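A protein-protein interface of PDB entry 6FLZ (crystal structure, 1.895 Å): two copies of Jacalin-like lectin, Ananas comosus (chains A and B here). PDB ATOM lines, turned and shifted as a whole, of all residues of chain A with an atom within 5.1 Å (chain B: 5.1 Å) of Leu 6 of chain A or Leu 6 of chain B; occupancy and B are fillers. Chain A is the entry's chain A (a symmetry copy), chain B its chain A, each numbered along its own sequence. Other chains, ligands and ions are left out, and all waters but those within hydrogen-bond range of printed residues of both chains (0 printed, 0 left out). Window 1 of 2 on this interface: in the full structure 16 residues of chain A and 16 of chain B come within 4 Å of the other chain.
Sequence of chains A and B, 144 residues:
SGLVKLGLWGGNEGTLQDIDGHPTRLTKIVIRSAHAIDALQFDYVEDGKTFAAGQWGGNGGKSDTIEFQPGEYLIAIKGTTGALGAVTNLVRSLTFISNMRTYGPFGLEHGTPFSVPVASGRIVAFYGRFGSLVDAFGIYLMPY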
ATOM      1  N   VAL A   4       4.768  16.855 -16.141  1.00  0.00           N
ATOM      2  CA  VAL A   4       5.435  16.639 -14.866  1.00  0.00           C
ATOM      3  C   VAL A   4       5.423  15.144 -14.589  1.00  0.00           C
ATOM      4  O   VAL A   4       4.382  14.486 -14.709  1.00  0.00           O
ATOM      5  CB  VAL A   4       4.738  17.427 -13.745  1.00  0.00           C
ATOM      6  CG1 VAL A   4       5.297  17.036 -12.376  1.00  0.00           C
ATOM      7  CG2 VAL A   4       4.880  18.928 -13.978  1.00  0.00           C
ATOM      8  N   LYS A   5       6.583  14.599 -14.242  1.00  0.00           N
ATOM      9  CA  LYS A   5       6.759  13.164 -14.030  1.00  0.00           C
ATOM     10  C   LYS A   5       7.123  12.941 -12.568  1.00  0.00           C
ATOM     11  O   LYS A   5       8.192  13.369 -12.118  1.00  0.00           O
ATOM     12  CB  LYS A   5       7.844  12.624 -14.957  1.00  0.00           C
ATOM     13  CG  LYS A   5       7.985  11.106 -15.007  1.00  0.00           C
ATOM     14  CD  LYS A   5       9.114  10.758 -15.976  1.00  0.00           C
ATOM     15  CE  LYS A   5       9.284   9.281 -16.174  1.00  0.00           C
ATOM     16  NZ  LYS A   5      10.306   9.006 -17.231  1.00  0.00           N
ATOM     17  N   LEU A   6       6.232  12.282 -11.830  1.00  0.00           N
ATOM     18  CA  LEU A   6       6.430  11.986 -10.417  1.00  0.00           C
ATOM     19  C   LEU A   6       6.757  10.513 -10.234  1.00  0.00           C
ATOM     20  O   LEU A   6       6.143   9.645 -10.864  1.00  0.00           O
ATOM     21  CB  LEU A   6       5.184  12.315  -9.593  1.00  0.00           C
ATOM     22  CG  LEU A   6       4.606  13.727  -9.695  1.00  0.00           C
ATOM     23  CD1 LEU A   6       3.368  13.836  -8.812  1.00  0.00           C
ATOM     24  CD2 LEU A   6       5.652  14.774  -9.301  1.00  0.00           C
ATOM     25  N   GLY A   7       7.697  10.236  -9.343  1.00  0.00           N
ATOM     26  CA  GLY A   7       8.085   8.870  -9.050  1.00  0.00           C
ATOM     27  C   GLY A   7       9.573   8.807  -8.794  1.00  0.00           C
ATOM     28  O   GLY A   7      10.252   9.836  -8.905  1.00  0.00           O
ATOM     29  N   LEU A   8      10.093   7.632  -8.441  1.00  0.00           N
ATOM     30  CA  LEU A   8       9.312   6.403  -8.271  1.00  0.00           C
ATOM     31  C   LEU A   8       8.925   6.141  -6.818  1.00  0.00           C
ATOM     32  O   LEU A   8       9.702   6.426  -5.910  1.00  0.00           O
ATOM     33  CB  LEU A   8      10.116   5.202  -8.769  1.00  0.00           C
ATOM     34  CG  LEU A   8      10.316   5.102 -10.275  1.00  0.00           C
ATOM     35  CD1 LEU A   8      11.412   4.099 -10.572  1.00  0.00           C
ATOM     36  CD2 LEU A   8       9.009   4.692 -10.941  1.00  0.00           C
ATOM     37  N   TRP A   9       7.737   5.577  -6.608  1.00  0.00           N
ATOM     38  CA  TRP A   9       7.360   4.998  -5.321  1.00  0.00           C
ATOM     39  C   TRP A   9       7.567   3.493  -5.393  1.00  0.00           C
ATOM     40  O   TRP A   9       7.042   2.834  -6.298  1.00  0.00           O
ATOM     41  CB  TRP A   9       5.904   5.306  -4.966  1.00  0.00           C
ATOM     42  CG  TRP A   9       5.605   6.748  -4.681  1.00  0.00           C
ATOM     43  CD1 TRP A   9       5.748   7.386  -3.490  1.00  0.00           C
ATOM     44  CD2 TRP A   9       5.102   7.724  -5.603  1.00  0.00           C
ATOM     45  NE1 TRP A   9       5.369   8.700  -3.605  1.00  0.00           N
ATOM     46  CE2 TRP A   9       4.968   8.932  -4.895  1.00  0.00           C
ATOM     47  CE3 TRP A   9       4.749   7.692  -6.959  1.00  0.00           C
ATOM     48  CZ2 TRP A   9       4.499  10.094  -5.490  1.00  0.00           C
ATOM     49  CZ3 TRP A   9       4.290   8.852  -7.552  1.00  0.00           C
ATOM     50  CH2 TRP A   9       4.164  10.038  -6.816  1.00  0.00           C
ATOM     51  N   VAL A 116      -1.185  11.121  -3.825  1.00  0.00           N
ATOM     52  CA  VAL A 116      -1.010  12.207  -4.786  1.00  0.00           C
ATOM     53  C   VAL A 116      -2.372  12.837  -5.046  1.00  0.00           C
ATOM     54  O   VAL A 116      -3.067  12.443  -5.991  1.00  0.00           O
ATOM     55  CB  VAL A 116      -0.367  11.711  -6.088  1.00  0.00           C
ATOM     56  CG1 VAL A 116      -0.075  12.885  -7.009  1.00  0.00           C
ATOM     57  CG2 VAL A 116       0.904  10.948  -5.785  1.00  0.00           C
ATOM     58  N   PRO A 117      -2.814  13.772  -4.208  1.00  0.00           N
ATOM     59  CA  PRO A 117      -4.020  14.543  -4.527  1.00  0.00           C
ATOM     60  C   PRO A 117      -3.677  15.642  -5.528  1.00  0.00           C
ATOM     61  O   PRO A 117      -2.663  16.330  -5.392  1.00  0.00           O
ATOM     62  CB  PRO A 117      -4.449  15.114  -3.170  1.00  0.00           C
ATOM     63  CG  PRO A 117      -3.168  15.241  -2.397  1.00  0.00           C
ATOM     64  CD  PRO A 117      -2.238  14.155  -2.907  1.00  0.00           C
ATOM     65  N   VAL A 118      -4.500  15.771  -6.564  1.00  0.00           N
ATOM     66  CA  VAL A 118      -4.258  16.717  -7.651  1.00  0.00           C
ATOM     67  C   VAL A 118      -5.263  17.848  -7.500  1.00  0.00           C
ATOM     68  O   VAL A 118      -6.468  17.649  -7.696  1.00  0.00           O
ATOM     69  CB  VAL A 118      -4.364  16.043  -9.026  1.00  0.00           C
ATOM     70  CG1 VAL A 118      -4.048  17.039 -10.151  1.00  0.00           C
ATOM     71  CG2 VAL A 118      -3.432  14.839  -9.089  1.00  0.00           C
ATOM     72  N   ALA A 119      -4.768  19.035  -7.133  1.00  0.00           N
ATOM     73  CA  ALA A 119      -5.623  20.214  -7.051  1.00  0.00           C
ATOM     74  C   ALA A 119      -5.846  20.849  -8.424  1.00  0.00           C
ATOM     75  O   ALA A 119      -6.946  21.325  -8.717  1.00  0.00           O
ATOM     76  CB  ALA A 119      -5.018  21.239  -6.093  1.00  0.00           C
ATOM     77  N   TYR A 127       4.416   5.142 -15.367  1.00  0.00           N
ATOM     78  CA  TYR A 127       5.598   4.335 -15.656  1.00  0.00           C
ATOM     79  C   TYR A 127       5.940   3.572 -14.375  1.00  0.00           C
ATOM     80  O   TYR A 127       5.255   3.709 -13.356  1.00  0.00           O
ATOM     81  CB  TYR A 127       6.763   5.204 -16.173  1.00  0.00           C
ATOM     82  CG  TYR A 127       7.485   6.025 -15.117  1.00  0.00           C
ATOM     83  CD1 TYR A 127       6.859   7.083 -14.474  1.00  0.00           C
ATOM     84  CD2 TYR A 127       8.799   5.742 -14.774  1.00  0.00           C
ATOM     85  CE1 TYR A 127       7.521   7.834 -13.511  1.00  0.00           C
ATOM     86  CE2 TYR A 127       9.467   6.478 -13.803  1.00  0.00           C
ATOM     87  CZ  TYR A 127       8.821   7.520 -13.169  1.00  0.00           C
ATOM     88  OH  TYR A 127       9.471   8.267 -12.203  1.00  0.00           O
ATOM     89  N   PHE A 137       6.352   2.494  -9.025  1.00  0.00           N
ATOM     90  CA  PHE A 137       5.240   3.138  -9.710  1.00  0.00           C
ATOM     91  C   PHE A 137       5.482   4.641  -9.814  1.00  0.00           C
ATOM     92  O   PHE A 137       6.046   5.252  -8.898  1.00  0.00           O
ATOM     93  CB  PHE A 137       3.940   2.826  -8.953  1.00  0.00           C
ATOM     94  CG  PHE A 137       2.733   3.569  -9.449  1.00  0.00           C
ATOM     95  CD1 PHE A 137       2.056   3.154 -10.586  1.00  0.00           C
ATOM     96  CD2 PHE A 137       2.248   4.656  -8.749  1.00  0.00           C
ATOM     97  CE1 PHE A 137       0.929   3.829 -11.021  1.00  0.00           C
ATOM     98  CE2 PHE A 137       1.123   5.340  -9.185  1.00  0.00           C
ATOM     99  CZ  PHE A 137       0.463   4.926 -10.318  1.00  0.00           C
ATOM    100  N   GLY A 138       5.059   5.227 -10.941  1.00  0.00           N
ATOM    101  CA  GLY A 138       5.152   6.662 -11.146  1.00  0.00           C
ATOM    102  C   GLY A 138       4.053   7.162 -12.063  1.00  0.00           C
ATOM    103  O   GLY A 138       3.350   6.380 -12.703  1.00  0.00           O
ATOM    104  N   ILE A 139       3.918   8.490 -12.115  1.00  0.00           N
ATOM    105  CA  ILE A 139       2.752   9.163 -12.686  1.00  0.00           C
ATOM    106  C   ILE A 139       3.207  10.315 -13.575  1.00  0.00           C
ATOM    107  O   ILE A 139       4.122  11.063 -13.214  1.00  0.00           O
ATOM    108  CB  ILE A 139       1.827   9.720 -11.580  1.00  0.00           C
ATOM    109  CG1 ILE A 139       1.383   8.624 -10.616  1.00  0.00           C
ATOM    110  CG2 ILE A 139       0.603  10.384 -12.188  1.00  0.00           C
ATOM    111  CD1 ILE A 139       0.788   9.186  -9.307  1.00  0.00           C
ATOM    112  N   TYR A 140       2.530  10.486 -14.714  1.00  0.00           N
ATOM    113  CA  TYR A 140       2.678  11.655 -15.577  1.00  0.00           C
ATOM    114  C   TYR A 140       1.475  12.578 -15.435  1.00  0.00           C
ATOM    115  O   TYR A 140       0.334  12.123 -15.566  1.00  0.00           O
ATOM    116  CB  TYR A 140       2.785  11.251 -17.048  1.00  0.00           C
ATOM    117  CG  TYR A 140       4.082  10.671 -17.486  1.00  0.00           C
ATOM    118  CD1 TYR A 140       5.110  11.490 -17.913  1.00  0.00           C
ATOM    119  CD2 TYR A 140       4.270   9.293 -17.534  1.00  0.00           C
ATOM    120  CE1 TYR A 140       6.310  10.959 -18.366  1.00  0.00           C
ATOM    121  CE2 TYR A 140       5.465   8.749 -17.981  1.00  0.00           C
ATOM    122  CZ  TYR A 140       6.483   9.593 -18.398  1.00  0.00           C
ATOM    123  OH  TYR A 140       7.677   9.068 -18.841  1.00  0.00           O
ATOM    124  N   LEU A 141       1.730  13.874 -15.225  1.00  0.00           N
ATOM    125  CA  LEU A 141       0.681  14.879 -15.118  1.00  0.00           C
ATOM    126  C   LEU A 141       0.879  16.011 -16.114  1.00  0.00           C
ATOM    127  O   LEU A 141       2.003  16.467 -16.348  1.00  0.00           O
ATOM    128  CB  LEU A 141       0.626  15.482 -13.715  1.00  0.00           C
ATOM    129  CG  LEU A 141       0.378  14.478 -12.599  1.00  0.00           C
ATOM    130  CD1 LEU A 141       1.697  14.071 -11.959  1.00  0.00           C
ATOM    131  CD2 LEU A 141      -0.573  15.061 -11.580  1.00  0.00           C
ATOM    132  N   VAL B   4       1.334  22.386 -12.515  1.00  0.00           N
ATOM    133  CA  VAL B   4       0.624  21.304 -11.850  1.00  0.00           C
ATOM    134  C   VAL B   4       0.598  21.618 -10.362  1.00  0.00           C
ATOM    135  O   VAL B   4       1.629  21.958  -9.769  1.00  0.00           O
ATOM    136  CB  VAL B   4       1.303  19.953 -12.130  1.00  0.00           C
ATOM    137  CG1 VAL B   4       0.695  18.848 -11.264  1.00  0.00           C
ATOM    138  CG2 VAL B   4       1.198  19.599 -13.610  1.00  0.00           C
ATOM    139  N   LYS B   5      -0.583  21.529  -9.762  1.00  0.00           N
ATOM    140  CA  LYS B   5      -0.795  21.884  -8.360  1.00  0.00           C
ATOM    141  C   LYS B   5      -1.207  20.625  -7.608  1.00  0.00           C
ATOM    142  O   LYS B   5      -2.280  20.067  -7.865  1.00  0.00           O
ATOM    143  CB  LYS B   5      -1.862  22.968  -8.247  1.00  0.00           C
ATOM    144  CG  LYS B   5      -2.032  23.596  -6.867  1.00  0.00           C
ATOM    145  CD  LYS B   5      -3.138  24.648  -6.949  1.00  0.00           C
ATOM    146  CE  LYS B   5      -3.331  25.398  -5.664  1.00  0.00           C
ATOM    147  NZ  LYS B   5      -4.326  26.500  -5.844  1.00  0.00           N
ATOM    148  N   LEU B   6      -0.352  20.176  -6.692  1.00  0.00           N
ATOM    149  CA  LEU B   6      -0.598  18.987  -5.886  1.00  0.00           C
ATOM    150  C   LEU B   6      -0.961  19.387  -4.464  1.00  0.00           C
ATOM    151  O   LEU B   6      -0.346  20.288  -3.883  1.00  0.00           O
ATOM    152  CB  LEU B   6       0.628  18.075  -5.838  1.00  0.00           C
ATOM    153  CG  LEU B   6       1.238  17.619  -7.165  1.00  0.00           C
ATOM    154  CD1 LEU B   6       2.451  16.736  -6.891  1.00  0.00           C
ATOM    155  CD2 LEU B   6       0.202  16.876  -8.013  1.00  0.00           C
ATOM    156  N   GLY B   7      -1.933  18.688  -3.897  1.00  0.00           N
ATOM    157  CA  GLY B   7      -2.357  18.947  -2.535  1.00  0.00           C
ATOM    158  C   GLY B   7      -3.853  18.764  -2.424  1.00  0.00           C
ATOM    159  O   GLY B   7      -4.507  18.487  -3.438  1.00  0.00           O
ATOM    160  N   LEU B   8      -4.407  18.896  -1.220  1.00  0.00           N
ATOM    161  CA  LEU B   8      -3.657  19.192   0.004  1.00  0.00           C
ATOM    162  C   LEU B   8      -3.319  17.941   0.811  1.00  0.00           C
ATOM    163  O   LEU B   8      -4.118  17.009   0.870  1.00  0.00           O
ATOM    164  CB  LEU B   8      -4.469  20.127   0.900  1.00  0.00           C
ATOM    165  CG  LEU B   8      -4.626  21.561   0.413  1.00  0.00           C
ATOM    166  CD1 LEU B   8      -5.733  22.241   1.194  1.00  0.00           C
ATOM    167  CD2 LEU B   8      -3.308  22.306   0.578  1.00  0.00           C
ATOM    168  N   TRP B   9      -2.151  17.939   1.449  1.00  0.00           N
ATOM    169  CA  TRP B   9      -1.824  16.962   2.485  1.00  0.00           C
ATOM    170  C   TRP B   9      -2.060  17.608   3.842  1.00  0.00           C
ATOM    171  O   TRP B   9      -1.521  18.684   4.123  1.00  0.00           O
ATOM    172  CB  TRP B   9      -0.373  16.487   2.380  1.00  0.00           C
ATOM    173  CG  TRP B   9      -0.054  15.668   1.165  1.00  0.00           C
ATOM    174  CD1 TRP B   9      -0.220  14.326   1.024  1.00  0.00           C
ATOM    175  CD2 TRP B   9       0.497  16.138  -0.073  1.00  0.00           C
ATOM    176  NE1 TRP B   9       0.188  13.924  -0.222  1.00  0.00           N
ATOM    177  CE2 TRP B   9       0.633  15.019  -0.916  1.00  0.00           C
ATOM    178  CE3 TRP B   9       0.889  17.396  -0.550  1.00  0.00           C
ATOM    179  CZ2 TRP B   9       1.144  15.116  -2.202  1.00  0.00           C
ATOM    180  CZ3 TRP B   9       1.390  17.491  -1.834  1.00  0.00           C
ATOM    181  CH2 TRP B   9       1.517  16.356  -2.646  1.00  0.00           C
ATOM    182  N   VAL B 116       6.794  13.071  -2.345  1.00  0.00           N
ATOM    183  CA  VAL B 116       6.670  13.548  -3.720  1.00  0.00           C
ATOM    184  C   VAL B 116       8.052  13.520  -4.359  1.00  0.00           C
ATOM    185  O   VAL B 116       8.767  14.530  -4.335  1.00  0.00           O
ATOM    186  CB  VAL B 116       6.057  14.954  -3.777  1.00  0.00           C
ATOM    187  CG1 VAL B 116       5.817  15.362  -5.222  1.00  0.00           C
ATOM    188  CG2 VAL B 116       4.762  14.990  -2.995  1.00  0.00           C
ATOM    189  N   PRO B 117       8.487  12.380  -4.892  1.00  0.00           N
ATOM    190  CA  PRO B 117       9.718  12.357  -5.689  1.00  0.00           C
ATOM    191  C   PRO B 117       9.428  12.870  -7.096  1.00  0.00           C
ATOM    192  O   PRO B 117       8.424  12.502  -7.711  1.00  0.00           O
ATOM    193  CB  PRO B 117      10.117  10.876  -5.687  1.00  0.00           C
ATOM    194  CG  PRO B 117       8.816  10.139  -5.549  1.00  0.00           C
ATOM    195  CD  PRO B 117       7.879  11.044  -4.768  1.00  0.00           C
ATOM    196  N   VAL B 118      10.284  13.761  -7.584  1.00  0.00           N
ATOM    197  CA  VAL B 118      10.094  14.410  -8.880  1.00  0.00           C
ATOM    198  C   VAL B 118      11.117  13.818  -9.837  1.00  0.00           C
ATOM    199  O   VAL B 118      12.323  14.051  -9.692  1.00  0.00           O
ATOM    200  CB  VAL B 118      10.228  15.935  -8.778  1.00  0.00           C
ATOM    201  CG1 VAL B 118       9.966  16.601 -10.136  1.00  0.00           C
ATOM    202  CG2 VAL B 118       9.274  16.472  -7.718  1.00  0.00           C
ATOM    203  N   ALA B 119      10.635  13.036 -10.810  1.00  0.00           N
ATOM    204  CA  ALA B 119      11.511  12.493 -11.843  1.00  0.00           C
ATOM    205  C   ALA B 119      11.789  13.515 -12.945  1.00  0.00           C
ATOM    206  O   ALA B 119      12.906  13.582 -13.464  1.00  0.00           O
ATOM    207  CB  ALA B 119      10.899  11.230 -12.443  1.00  0.00           C
ATOM    208  N   TYR B 127       1.425  26.132  -1.385  1.00  0.00           N
ATOM    209  CA  TYR B 127       0.236  26.731  -0.785  1.00  0.00           C
ATOM    210  C   TYR B 127      -0.160  25.845   0.398  1.00  0.00           C
ATOM    211  O   TYR B 127       0.496  24.837   0.680  1.00  0.00           O
ATOM    212  CB  TYR B 127      -0.895  26.900  -1.820  1.00  0.00           C
ATOM    213  CG  TYR B 127      -1.631  25.627  -2.198  1.00  0.00           C
ATOM    214  CD1 TYR B 127      -1.004  24.616  -2.912  1.00  0.00           C
ATOM    215  CD2 TYR B 127      -2.961  25.444  -1.845  1.00  0.00           C
ATOM    216  CE1 TYR B 127      -1.679  23.452  -3.260  1.00  0.00           C
ATOM    217  CE2 TYR B 127      -3.643  24.279  -2.176  1.00  0.00           C
ATOM    218  CZ  TYR B 127      -2.996  23.282  -2.879  1.00  0.00           C
ATOM    219  OH  TYR B 127      -3.659  22.118  -3.221  1.00  0.00           O
ATOM    220  N   PHE B 137      -0.755  21.320   3.419  1.00  0.00           N
ATOM    221  CA  PHE B 137       0.389  21.685   2.597  1.00  0.00           C
ATOM    222  C   PHE B 137       0.181  21.213   1.161  1.00  0.00           C
ATOM    223  O   PHE B 137      -0.398  20.145   0.927  1.00  0.00           O
ATOM    224  CB  PHE B 137       1.659  21.078   3.213  1.00  0.00           C
ATOM    225  CG  PHE B 137       2.896  21.229   2.374  1.00  0.00           C
ATOM    226  CD1 PHE B 137       3.599  22.424   2.345  1.00  0.00           C
ATOM    227  CD2 PHE B 137       3.381  20.157   1.650  1.00  0.00           C
ATOM    228  CE1 PHE B 137       4.751  22.546   1.590  1.00  0.00           C
ATOM    229  CE2 PHE B 137       4.533  20.276   0.886  1.00  0.00           C
ATOM    230  CZ  PHE B 137       5.218  21.468   0.858  1.00  0.00           C
ATOM    231  N   GLY B 138       0.650  22.022   0.203  1.00  0.00           N
ATOM    232  CA  GLY B 138       0.592  21.666  -1.204  1.00  0.00           C
ATOM    233  C   GLY B 138       1.728  22.301  -1.982  1.00  0.00           C
ATOM    234  O   GLY B 138       2.435  23.175  -1.482  1.00  0.00           O
ATOM    235  N   ILE B 139       1.892  21.839  -3.225  1.00  0.00           N
ATOM    236  CA  ILE B 139       3.088  22.087  -4.029  1.00  0.00           C
ATOM    237  C   ILE B 139       2.684  22.478  -5.446  1.00  0.00           C
ATOM    238  O   ILE B 139       1.773  21.878  -6.027  1.00  0.00           O
ATOM    239  CB  ILE B 139       3.991  20.833  -4.095  1.00  0.00           C
ATOM    240  CG1 ILE B 139       4.383  20.351  -2.701  1.00  0.00           C
ATOM    241  CG2 ILE B 139       5.246  21.117  -4.903  1.00  0.00           C
ATOM    242  CD1 ILE B 139       4.949  18.915  -2.704  1.00  0.00           C
ATOM    243  N   TYR B 140       3.399  23.452  -6.018  1.00  0.00           N
ATOM    244  CA  TYR B 140       3.300  23.806  -7.431  1.00  0.00           C
ATOM    245  C   TYR B 140       4.517  23.299  -8.193  1.00  0.00           C
ATOM    246  O   TYR B 140       5.652  23.570  -7.788  1.00  0.00           O
ATOM    247  CB  TYR B 140       3.230  25.321  -7.621  1.00  0.00           C
ATOM    248  CG  TYR B 140       1.935  25.974  -7.291  1.00  0.00           C
ATOM    249  CD1 TYR B 140       0.938  26.077  -8.242  1.00  0.00           C
ATOM    250  CD2 TYR B 140       1.720  26.548  -6.041  1.00  0.00           C
ATOM    251  CE1 TYR B 140      -0.259  26.723  -7.959  1.00  0.00           C
ATOM    252  CE2 TYR B 140       0.529  27.193  -5.745  1.00  0.00           C
ATOM    253  CZ  TYR B 140      -0.458  27.277  -6.715  1.00  0.00           C
ATOM    254  OH  TYR B 140      -1.649  27.911  -6.434  1.00  0.00           O
ATOM    255  N   LEU B 141       4.282  22.615  -9.319  1.00  0.00           N
ATOM    256  CA  LEU B 141       5.348  22.111 -10.175  1.00  0.00           C
ATOM    257  C   LEU B 141       5.202  22.604 -11.606  1.00  0.00           C
ATOM    258  O   LEU B 141       4.096  22.669 -12.151  1.00  0.00           O
ATOM    259  CB  LEU B 141       5.372  20.584 -10.196  1.00  0.00           C
ATOM    260  CG  LEU B 141       5.566  19.931  -8.836  1.00  0.00           C
ATOM    261  CD1 LEU B 141       4.220  19.521  -8.256  1.00  0.00           C
ATOM    262  CD2 LEU B 141       6.497  18.747  -8.958  1.00  0.00           C
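The backbone NH (N) of Ala 119 of chain B sits at hydrogen-bond distance from the backbone carbonyl oxygen (O) of Lys 5 of chain A (2.8 Å).
The backbone carbonyl oxygen of Lys 5 of chain B lies within hydrogen-bond range of the backbone NH of Ala 119 of chain A (2.8 Å).
N of Gly 7 of chain B is in hydrogen-bond range of O of Pro 117 of chain A.
N of Gly 7 of chain A sits at hydrogen-bond distance from O of Pro 117 of chain B (2.9 Å).
The backbone carbonyl oxygen (O) of Leu 6 of chain B lies within hydrogen-bond range of the backbone NH (N) of Ile 139 of chain B, 2.8 Å away.
O of Val 4 of chain A lies within hydrogen-bond range of N of Leu 141 of chain A.
The backbone NH (N) of Phe 137 of chain A sits at hydrogen-bond distance from the backbone carbonyl oxygen (O) of Trp 9 of chain A (2.8 Å).
The backbone carbonyl oxygen of Tyr 127 of chain A sits at hydrogen-bond distance from the backbone NH of Gly 138 of chain A (2.9 Å).
O of Trp 9 of chain B sits at hydrogen-bond distance from N of Phe 137 of chain B (2.8 Å).
The backbone carbonyl oxygen of Leu 6 of chain A lies within hydrogen-bond range of the backbone NH of Ile 139 of chain A (2.8 Å).
Among the printed residues, merely in contact across the chains: Val 4 of chain A with Val 4 of chain B, Lys 5 of chain A with Val 118 of chain B, Leu 6 of chain A with Leu 6 of chain B, Leu 6 of chain A with Pro 117 of chain B, Gly 7 of chain A with Ala 119 of chain B, Leu 8 of chain A with Pro 117 of chain B, Trp 9 of chain A with Pro 117 of chain B, Pro 117 of chain A with Leu 6 of chain B, Pro 117 of chain A with Leu 8 of chain B, Pro 117 of chain A with Trp 9 of chain B, Val 118 of chain A with Lys 5 of chain B, Ala 119 of chain A with Gly 7 of chain B, Ala 119 of chain A with Tyr 127 of chain B and Tyr 127 of chain A with Ala 119 of chain B.
Of the printed residues of chain B, Val 4 of chain A touches Val 4.
Of the printed residues of chain B, Val 118 of chain A touches Lys 5 (3.7 Å).
Of the printed residues of chain A, Val 4 of chain B touches Val 4.
Leu 6 of chain B touches two residues of chain A.
Of the printed residues of chain A, Leu 8 of chain B touches Pro 117.
Of the printed residues of chain A, Tyr 127 of chain B touches Ala 119.
Printed residues of chain A that touch a printed residue of chain B: Val 4, Lys 5, Leu 6, Gly 7, Leu 8, Trp 9, Pro 117, Val 118, Ala 119 and Tyr 127.
Of the 16 printed residues of chain B, 10 touch a printed residue of chain A.
Hydrophobic or aromatic side chains of chain B within 4 Å of the printed part of chain A: Val 4, Leu 6, Trp 9, Pro 117, Ala 119 and Tyr 127.
Among the printed residues, 18 pairs touch across the chains.
Lys 5 of chain A touches Ala 119 of chain B, and with the chains exchanged Ala 119 of chain A touches Lys 5 of chain B.
Leu 6 of chain B touches its own counterpart, Leu 6 of chain A.
Gly 7 of chain A touches Ala 119 of chain B, and with the chains exchanged Ala 119 of chain A touches Gly 7 of chain B.
Trp 9 of chain A touches Pro 117 of chain B, and with the chains exchanged Pro 117 of chain A touches Trp 9 of chain B.
Positions printed for both chains: 4, 5, 6, 7, 8, 9, 116, 117, 118, 119, 127, 137, 138, 139, 140 and 141.
Of the 18 pairs that touch across the chains among the printed residues, 18 have their exchanged pair printed and touching as well.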
